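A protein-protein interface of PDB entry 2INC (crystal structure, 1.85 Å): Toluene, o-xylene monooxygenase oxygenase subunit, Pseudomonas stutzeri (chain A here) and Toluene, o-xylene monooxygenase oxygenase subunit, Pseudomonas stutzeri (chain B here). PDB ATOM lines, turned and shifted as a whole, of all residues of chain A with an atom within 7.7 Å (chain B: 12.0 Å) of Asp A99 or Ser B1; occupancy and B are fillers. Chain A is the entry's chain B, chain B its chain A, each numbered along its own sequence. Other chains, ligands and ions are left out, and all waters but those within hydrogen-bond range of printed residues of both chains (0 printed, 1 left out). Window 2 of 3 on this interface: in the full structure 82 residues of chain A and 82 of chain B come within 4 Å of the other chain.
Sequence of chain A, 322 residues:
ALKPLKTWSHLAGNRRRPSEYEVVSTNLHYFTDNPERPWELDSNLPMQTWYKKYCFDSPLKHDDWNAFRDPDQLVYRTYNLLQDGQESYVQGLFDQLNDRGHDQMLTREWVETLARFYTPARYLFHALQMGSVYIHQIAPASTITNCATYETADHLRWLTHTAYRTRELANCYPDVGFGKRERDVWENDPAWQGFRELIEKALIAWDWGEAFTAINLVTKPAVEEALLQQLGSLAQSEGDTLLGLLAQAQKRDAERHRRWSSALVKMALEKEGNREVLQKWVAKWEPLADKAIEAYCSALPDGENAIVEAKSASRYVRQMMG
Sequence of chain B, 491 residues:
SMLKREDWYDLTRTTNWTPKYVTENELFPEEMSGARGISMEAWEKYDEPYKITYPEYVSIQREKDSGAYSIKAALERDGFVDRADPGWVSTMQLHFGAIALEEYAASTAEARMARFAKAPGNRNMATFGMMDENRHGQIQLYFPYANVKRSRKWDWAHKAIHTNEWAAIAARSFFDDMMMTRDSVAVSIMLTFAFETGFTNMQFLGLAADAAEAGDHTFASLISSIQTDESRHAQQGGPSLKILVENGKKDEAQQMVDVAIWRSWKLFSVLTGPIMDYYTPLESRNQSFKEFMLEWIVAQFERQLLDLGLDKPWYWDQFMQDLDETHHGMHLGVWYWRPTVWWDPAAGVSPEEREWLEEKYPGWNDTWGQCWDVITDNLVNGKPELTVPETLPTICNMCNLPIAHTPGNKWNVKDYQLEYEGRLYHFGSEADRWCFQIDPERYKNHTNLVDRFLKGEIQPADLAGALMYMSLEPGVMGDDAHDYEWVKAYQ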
ATOM      1  N   GLN A  91     -25.141  14.621  23.579  1.00  0.00           N
ATOM      2  CA  GLN A  91     -24.326  14.357  22.407  1.00  0.00           C
ATOM      3  C   GLN A  91     -24.458  12.877  21.996  1.00  0.00           C
ATOM      4  O   GLN A  91     -24.463  12.580  20.811  1.00  0.00           O
ATOM      5  CB  GLN A  91     -22.869  14.871  22.539  1.00  0.00           C
ATOM      6  CG  GLN A  91     -22.769  16.364  23.105  1.00  0.00           C
ATOM      7  CD  GLN A  91     -23.211  17.530  22.133  1.00  0.00           C
ATOM      8  OE1 GLN A  91     -22.814  17.577  20.962  1.00  0.00           O
ATOM      9  NE2 GLN A  91     -24.022  18.472  22.644  1.00  0.00           N
ATOM     10  N   GLY A  92     -24.682  11.978  22.957  1.00  0.00           N
ATOM     11  CA  GLY A  92     -24.994  10.632  22.597  1.00  0.00           C
ATOM     12  C   GLY A  92     -26.281  10.542  21.804  1.00  0.00           C
ATOM     13  O   GLY A  92     -26.321   9.826  20.801  1.00  0.00           O
ATOM     14  N   LEU A  93     -27.346  11.209  22.277  1.00  0.00           N
ATOM     15  CA  LEU A  93     -28.621  11.261  21.544  1.00  0.00           C
ATOM     16  C   LEU A  93     -28.421  11.735  20.152  1.00  0.00           C
ATOM     17  O   LEU A  93     -28.925  11.117  19.220  1.00  0.00           O
ATOM     18  CB  LEU A  93     -29.630  12.215  22.155  1.00  0.00           C
ATOM     19  CG  LEU A  93     -30.369  11.622  23.345  1.00  0.00           C
ATOM     20  CD1 LEU A  93     -31.294  12.678  24.021  1.00  0.00           C
ATOM     21  CD2 LEU A  93     -31.145  10.363  22.875  1.00  0.00           C
ATOM     22  N   PHE A  94     -27.722  12.847  19.995  1.00  0.00           N
ATOM     23  CA  PHE A  94     -27.458  13.364  18.645  1.00  0.00           C
ATOM     24  C   PHE A  94     -26.744  12.307  17.806  1.00  0.00           C
ATOM     25  O   PHE A  94     -27.064  12.104  16.628  1.00  0.00           O
ATOM     26  CB  PHE A  94     -26.591  14.609  18.705  1.00  0.00           C
ATOM     27  CG  PHE A  94     -27.302  15.847  19.274  1.00  0.00           C
ATOM     28  CD1 PHE A  94     -26.585  17.037  19.438  1.00  0.00           C
ATOM     29  CD2 PHE A  94     -28.648  15.811  19.635  1.00  0.00           C
ATOM     30  CE1 PHE A  94     -27.179  18.160  19.935  1.00  0.00           C
ATOM     31  CE2 PHE A  94     -29.276  16.971  20.166  1.00  0.00           C
ATOM     32  CZ  PHE A  94     -28.529  18.142  20.283  1.00  0.00           C
ATOM     33  N   ASP A  95     -25.734  11.661  18.400  1.00  0.00           N
ATOM     34  CA  ASP A  95     -24.896  10.746  17.623  1.00  0.00           C
ATOM     35  C   ASP A  95     -25.727   9.538  17.263  1.00  0.00           C
ATOM     36  O   ASP A  95     -25.747   9.108  16.147  1.00  0.00           O
ATOM     37  CB  ASP A  95     -23.693  10.353  18.460  1.00  0.00           C
ATOM     38  CG  ASP A  95     -22.718   9.424  17.763  1.00  0.00           C
ATOM     39  OD1 ASP A  95     -22.551   9.477  16.515  1.00  0.00           O
ATOM     40  OD2 ASP A  95     -21.986   8.730  18.528  1.00  0.00           O
ATOM     41  N   GLN A  96     -26.411   8.962  18.244  1.00  0.00           N
ATOM     42  CA  GLN A  96     -27.065   7.683  18.021  1.00  0.00           C
ATOM     43  C   GLN A  96     -28.367   7.807  17.199  1.00  0.00           C
ATOM     44  O   GLN A  96     -28.696   6.917  16.404  1.00  0.00           O
ATOM     45  CB  GLN A  96     -27.139   6.940  19.388  1.00  0.00           C
ATOM     46  CG  GLN A  96     -25.629   6.634  19.750  1.00  0.00           C
ATOM     47  CD  GLN A  96     -25.402   5.581  20.797  1.00  0.00           C
ATOM     48  OE1 GLN A  96     -26.023   4.541  20.756  1.00  0.00           O
ATOM     49  NE2 GLN A  96     -24.426   5.833  21.730  1.00  0.00           N
ATOM     50  N   LEU A  97     -29.045   8.958  17.282  1.00  0.00           N
ATOM     51  CA  LEU A  97     -30.281   9.143  16.525  1.00  0.00           C
ATOM     52  C   LEU A  97     -29.944   9.463  15.054  1.00  0.00           C
ATOM     53  O   LEU A  97     -30.662   9.021  14.154  1.00  0.00           O
ATOM     54  CB  LEU A  97     -31.223  10.169  17.208  1.00  0.00           C
ATOM     55  CG  LEU A  97     -31.966   9.570  18.423  1.00  0.00           C
ATOM     56  CD1 LEU A  97     -32.735  10.637  19.205  1.00  0.00           C
ATOM     57  CD2 LEU A  97     -32.933   8.492  17.978  1.00  0.00           C
ATOM     58  N   ASN A  98     -28.825  10.140  14.802  1.00  0.00           N
ATOM     59  CA  ASN A  98     -28.367  10.357  13.450  1.00  0.00           C
ATOM     60  C   ASN A  98     -28.047   8.999  12.825  1.00  0.00           C
ATOM     61  O   ASN A  98     -28.339   8.734  11.635  1.00  0.00           O
ATOM     62  CB  ASN A  98     -27.115  11.200  13.472  1.00  0.00           C
ATOM     63  CG  ASN A  98     -26.467  11.275  12.159  1.00  0.00           C
ATOM     64  OD1 ASN A  98     -26.799  12.122  11.318  1.00  0.00           O
ATOM     65  ND2 ASN A  98     -25.566  10.397  11.929  1.00  0.00           N
ATOM     66  N   ASP A  99     -27.480   8.121  13.645  1.00  0.00           N
ATOM     67  CA  ASP A  99     -27.073   6.794  13.162  1.00  0.00           C
ATOM     68  C   ASP A  99     -27.998   5.844  12.379  1.00  0.00           C
ATOM     69  O   ASP A  99     -27.767   5.665  11.200  1.00  0.00           O
ATOM     70  CB  ASP A  99     -26.339   5.977  14.239  1.00  0.00           C
ATOM     71  CG  ASP A  99     -24.831   6.239  14.286  1.00  0.00           C
ATOM     72  OD1 ASP A  99     -24.270   5.895  15.342  1.00  0.00           O
ATOM     73  OD2 ASP A  99     -24.181   6.754  13.317  1.00  0.00           O
ATOM     74  N   ARG A 100     -29.030   5.207  12.893  1.00  0.00           N
ATOM     75  CA  ARG A 100     -30.421   5.591  13.071  1.00  0.00           C
ATOM     76  C   ARG A 100     -31.245   6.275  11.981  1.00  0.00           C
ATOM     77  O   ARG A 100     -32.282   5.745  11.608  1.00  0.00           O
ATOM     78  CB  ARG A 100     -30.836   5.960  14.440  1.00  0.00           C
ATOM     79  CG  ARG A 100     -32.254   5.586  14.587  1.00  0.00           C
ATOM     80  CD  ARG A 100     -32.445   4.815  15.836  1.00  0.00           C
ATOM     81  NE  ARG A 100     -33.642   5.287  16.478  1.00  0.00           N
ATOM     82  CZ  ARG A 100     -34.165   4.738  17.563  1.00  0.00           C
ATOM     83  NH1 ARG A 100     -35.270   5.258  18.091  1.00  0.00           N
ATOM     84  NH2 ARG A 100     -33.584   3.667  18.097  1.00  0.00           N
ATOM     85  N   GLY A 101     -30.825   7.434  11.496  1.00  0.00           N
ATOM     86  CA  GLY A 101     -31.614   8.132  10.473  1.00  0.00           C
ATOM     87  C   GLY A 101     -32.934   8.736  10.958  1.00  0.00           C
ATOM     88  O   GLY A 101     -33.883   8.845  10.176  1.00  0.00           O
ATOM     89  N   HIS A 102     -32.985   9.152  12.234  1.00  0.00           N
ATOM     90  CA  HIS A 102     -34.163   9.802  12.840  1.00  0.00           C
ATOM     91  C   HIS A 102     -34.774  10.978  12.025  1.00  0.00           C
ATOM     92  O   HIS A 102     -35.992  11.114  11.896  1.00  0.00           O
ATOM     93  CB  HIS A 102     -33.745  10.298  14.241  1.00  0.00           C
ATOM     94  CG  HIS A 102     -34.704  11.247  14.873  1.00  0.00           C
ATOM     95  ND1 HIS A 102     -34.745  12.598  14.565  1.00  0.00           N
ATOM     96  CD2 HIS A 102     -35.663  11.042  15.805  1.00  0.00           C
ATOM     97  CE1 HIS A 102     -35.714  13.172  15.256  1.00  0.00           C
ATOM     98  NE2 HIS A 102     -36.267  12.259  16.040  1.00  0.00           N
ATOM     99  N   GLN A 104     -34.617  11.685   8.847  1.00  0.00           N
ATOM    100  CA  GLN A 104     -35.196  11.140   7.589  1.00  0.00           C
ATOM    101  C   GLN A 104     -36.598  10.593   7.774  1.00  0.00           C
ATOM    102  O   GLN A 104     -37.350  10.513   6.817  1.00  0.00           O
ATOM    103  CB  GLN A 104     -34.267  10.044   7.002  1.00  0.00           C
ATOM    104  CG  GLN A 104     -32.919  10.564   6.388  1.00  0.00           C
ATOM    105  CD  GLN A 104     -31.830  11.064   7.418  1.00  0.00           C
ATOM    106  OE1 GLN A 104     -30.917  11.835   7.047  1.00  0.00           O
ATOM    107  NE2 GLN A 104     -31.926  10.620   8.695  1.00  0.00           N
ATOM    108  N   TYR A 164     -26.518  23.360  16.360  1.00  0.00           N
ATOM    109  CA  TYR A 164     -26.101  22.058  15.853  1.00  0.00           C
ATOM    110  C   TYR A 164     -27.228  21.358  15.090  1.00  0.00           C
ATOM    111  O   TYR A 164     -27.079  20.922  13.909  1.00  0.00           O
ATOM    112  CB  TYR A 164     -25.681  21.178  17.085  1.00  0.00           C
ATOM    113  CG  TYR A 164     -25.149  19.820  16.630  1.00  0.00           C
ATOM    114  CD1 TYR A 164     -23.799  19.640  16.448  1.00  0.00           C
ATOM    115  CD2 TYR A 164     -26.018  18.725  16.403  1.00  0.00           C
ATOM    116  CE1 TYR A 164     -23.266  18.435  16.033  1.00  0.00           C
ATOM    117  CE2 TYR A 164     -25.497  17.474  15.973  1.00  0.00           C
ATOM    118  CZ  TYR A 164     -24.098  17.365  15.797  1.00  0.00           C
ATOM    119  OH  TYR A 164     -23.495  16.183  15.358  1.00  0.00           O
ATOM    120  N   GLU A 168     -27.895  20.057  11.143  1.00  0.00           N
ATOM    121  CA  GLU A 168     -28.293  18.676  10.821  1.00  0.00           C
ATOM    122  C   GLU A 168     -29.588  18.625  10.041  1.00  0.00           C
ATOM    123  O   GLU A 168     -29.719  17.871   9.048  1.00  0.00           O
ATOM    124  CB  GLU A 168     -28.456  17.853  12.100  1.00  0.00           C
ATOM    125  CG  GLU A 168     -27.180  17.489  12.743  1.00  0.00           C
ATOM    126  CD  GLU A 168     -27.324  16.184  13.490  1.00  0.00           C
ATOM    127  OE1 GLU A 168     -26.562  15.224  13.186  1.00  0.00           O
ATOM    128  OE2 GLU A 168     -28.232  16.097  14.362  1.00  0.00           O
ATOM    129  N   SER B   1     -23.669   9.526  13.790  1.00  0.00           N
ATOM    130  CA  SER B   1     -22.455  10.272  13.489  1.00  0.00           C
ATOM    131  C   SER B   1     -22.660  11.699  13.969  1.00  0.00           C
ATOM    132  O   SER B   1     -23.808  12.119  14.182  1.00  0.00           O
ATOM    133  CB  SER B   1     -22.156  10.299  11.983  1.00  0.00           C
ATOM    134  OG  SER B   1     -22.065   8.973  11.469  1.00  0.00           O
ATOM    135  N   MET B   2     -21.542  12.390  14.164  1.00  0.00           N
ATOM    136  CA  MET B   2     -21.515  13.823  14.561  1.00  0.00           C
ATOM    137  C   MET B   2     -21.051  14.683  13.405  1.00  0.00           C
ATOM    138  O   MET B   2     -20.179  14.262  12.623  1.00  0.00           O
ATOM    139  CB  MET B   2     -20.547  14.057  15.728  1.00  0.00           C
ATOM    140  CG  MET B   2     -20.788  13.266  16.994  1.00  0.00           C
ATOM    141  SD  MET B   2     -22.402  13.558  17.735  1.00  0.00           S
ATOM    142  CE  MET B   2     -22.214  15.113  18.624  1.00  0.00           C
ATOM    143  N   LEU B   3     -21.590  15.905  13.306  1.00  0.00           N
ATOM    144  CA  LEU B   3     -21.005  16.869  12.382  1.00  0.00           C
ATOM    145  C   LEU B   3     -19.592  17.282  12.822  1.00  0.00           C
ATOM    146  O   LEU B   3     -19.209  17.150  13.994  1.00  0.00           O
ATOM    147  CB  LEU B   3     -21.865  18.157  12.308  1.00  0.00           C
ATOM    148  CG  LEU B   3     -23.351  18.078  11.923  1.00  0.00           C
ATOM    149  CD1 LEU B   3     -24.069  19.366  12.385  1.00  0.00           C
ATOM    150  CD2 LEU B   3     -23.521  17.910  10.444  1.00  0.00           C
ATOM    151  N   LYS B   4     -18.846  17.826  11.863  1.00  0.00           N
ATOM    152  CA  LYS B   4     -17.554  18.484  12.101  1.00  0.00           C
ATOM    153  C   LYS B   4     -17.876  19.886  12.601  1.00  0.00           C
ATOM    154  O   LYS B   4     -18.809  20.480  12.097  1.00  0.00           O
ATOM    155  CB  LYS B   4     -16.870  18.631  10.749  1.00  0.00           C
ATOM    156  CG  LYS B   4     -16.869  17.363   9.886  1.00  0.00           C
ATOM    157  CD  LYS B   4     -15.979  17.526   8.650  1.00  0.00           C
ATOM    158  CE  LYS B   4     -14.510  17.790   9.066  1.00  0.00           C
ATOM    159  NZ  LYS B   4     -13.936  16.890  10.151  1.00  0.00           N
ATOM    160  N   ARG B   5     -17.117  20.404  13.574  1.00  0.00           N
ATOM    161  CA  ARG B   5     -17.387  21.692  14.172  1.00  0.00           C
ATOM    162  C   ARG B   5     -17.556  22.788  13.132  1.00  0.00           C
ATOM    163  O   ARG B   5     -18.408  23.679  13.256  1.00  0.00           O
ATOM    164  CB  ARG B   5     -16.256  22.091  15.113  1.00  0.00           C
ATOM    165  CG  ARG B   5     -16.582  23.407  15.826  1.00  0.00           C
ATOM    166  CD  ARG B   5     -15.607  23.776  16.898  1.00  0.00           C
ATOM    167  NE  ARG B   5     -14.314  24.138  16.364  1.00  0.00           N
ATOM    168  CZ  ARG B   5     -13.215  24.134  17.096  1.00  0.00           C
ATOM    169  NH1 ARG B   5     -13.278  23.749  18.355  1.00  0.00           N
ATOM    170  NH2 ARG B   5     -12.057  24.487  16.571  1.00  0.00           N
ATOM    171  N   GLU B   6     -16.707  22.723  12.112  1.00  0.00           N
ATOM    172  CA  GLU B   6     -16.606  23.784  11.152  1.00  0.00           C
ATOM    173  C   GLU B   6     -17.892  23.895  10.349  1.00  0.00           C
ATOM    174  O   GLU B   6     -18.202  24.946   9.821  1.00  0.00           O
ATOM    175  CB  GLU B   6     -15.401  23.564  10.226  1.00  0.00           C
ATOM    176  CG  GLU B   6     -14.995  22.048   9.964  1.00  0.00           C
ATOM    177  CD  GLU B   6     -14.369  21.282  11.222  1.00  0.00           C
ATOM    178  OE1 GLU B   6     -14.603  20.067  11.353  1.00  0.00           O
ATOM    179  OE2 GLU B   6     -13.643  21.860  12.068  1.00  0.00           O
ATOM    180  N   ASP B   7     -18.637  22.800  10.253  1.00  0.00           N
ATOM    181  CA  ASP B   7     -19.878  22.809   9.489  1.00  0.00           C
ATOM    182  C   ASP B   7     -21.033  23.540  10.151  1.00  0.00           C
ATOM    183  O   ASP B   7     -21.935  23.987   9.454  1.00  0.00           O
ATOM    184  CB  ASP B   7     -20.288  21.387   9.164  1.00  0.00           C
ATOM    185  CG  ASP B   7     -19.252  20.703   8.302  1.00  0.00           C
ATOM    186  OD1 ASP B   7     -18.552  21.428   7.492  1.00  0.00           O
ATOM    187  OD2 ASP B   7     -19.153  19.462   8.427  1.00  0.00           O
ATOM    188  N   TRP B   8     -21.003  23.694  11.487  1.00  0.00           N
ATOM    189  CA  TRP B   8     -22.124  24.335  12.172  1.00  0.00           C
ATOM    190  C   TRP B   8     -21.739  25.521  13.083  1.00  0.00           C
ATOM    191  O   TRP B   8     -22.613  26.218  13.628  1.00  0.00           O
ATOM    192  CB  TRP B   8     -22.891  23.300  13.008  1.00  0.00           C
ATOM    193  CG  TRP B   8     -22.114  22.628  14.106  1.00  0.00           C
ATOM    194  CD1 TRP B   8     -21.272  21.559  13.989  1.00  0.00           C
ATOM    195  CD2 TRP B   8     -22.110  22.998  15.486  1.00  0.00           C
ATOM    196  NE1 TRP B   8     -20.744  21.219  15.213  1.00  0.00           N
ATOM    197  CE2 TRP B   8     -21.259  22.090  16.157  1.00  0.00           C
ATOM    198  CE3 TRP B   8     -22.800  23.984  16.229  1.00  0.00           C
ATOM    199  CZ2 TRP B   8     -21.041  22.147  17.540  1.00  0.00           C
ATOM    200  CZ3 TRP B   8     -22.567  24.068  17.601  1.00  0.00           C
ATOM    201  CH2 TRP B   8     -21.716  23.129  18.250  1.00  0.00           C
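The side-chain carboxylate (OD2) of Asp A99 is in hydrogen-bond range of the backbone NH (N) of Ser B1 (2.9 Å).
The side-chain sulfur (SD) of Met B2 lies close to the side-chain hydroxyl (OH) of Tyr A164 (3.7 Å).
N of Leu B3 sits at hydrogen-bond distance from OH of Tyr A164 (2.8 Å).
N of Ser B1 sits close to ND2 of Asn A98 (2.8 Å).
The side-chain carboxylate of Asp A95 sits at hydrogen-bond distance from the backbone NH of Ser B1 (2.9 Å).
No residue of chain B comes within 4 Å of Gln A96.
Asn A98 touches just one residue of chain B: Ser B1.
Of the printed residues of chain B, Asp A99 touches Ser B1 (2.9 Å).
Gln A104 touches none of the printed residues of chain B.
Printed residues of chain B within 4 Å of Tyr A164: Met B2 (3.2 Å), Leu B3 (2.8 Å) and Trp B8 (3.5 Å).
Printed residues of chain B within 4 Å of Glu A168: Leu B3.
Ser B1 touches just these residues of chain A: Asp A95 (2.9 Å), Asn A98 (2.8 Å) and Asp A99 (2.9 Å).
Printed residues of chain A within 4 Å of Met B2: Gln A91 (3.4 Å), Asp A95 (3.5 Å) and Tyr A164 (3.2 Å).
Printed residues of chain A within 4 Å of Leu B3: Tyr A164 (2.8 Å) and Glu A168 (3.7 Å).
Printed residues of chain A within 4 Å of Trp B8: Tyr A164 (3.5 Å).
Gln A91 touches Met B2 (OE1 to CE, 3.4 Å).
Asp A95 touches Met B2 (CB to SD, 3.5 Å).
CD1 of Tyr A164 touches CE2 of Trp B8 (3.5 Å).
Leu B3 touches Glu A168.
Printed residues of chain A that touch a printed residue of chain B: Gln A91, Asp A95, Asn A98, Asp A99, Tyr A164 and Glu A168.
Hydrophobic or aromatic side chains of chain A that line the printed part of chain B: Tyr A164.
Of the 8 printed residues of chain B, 4 touch a printed residue of chain A.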
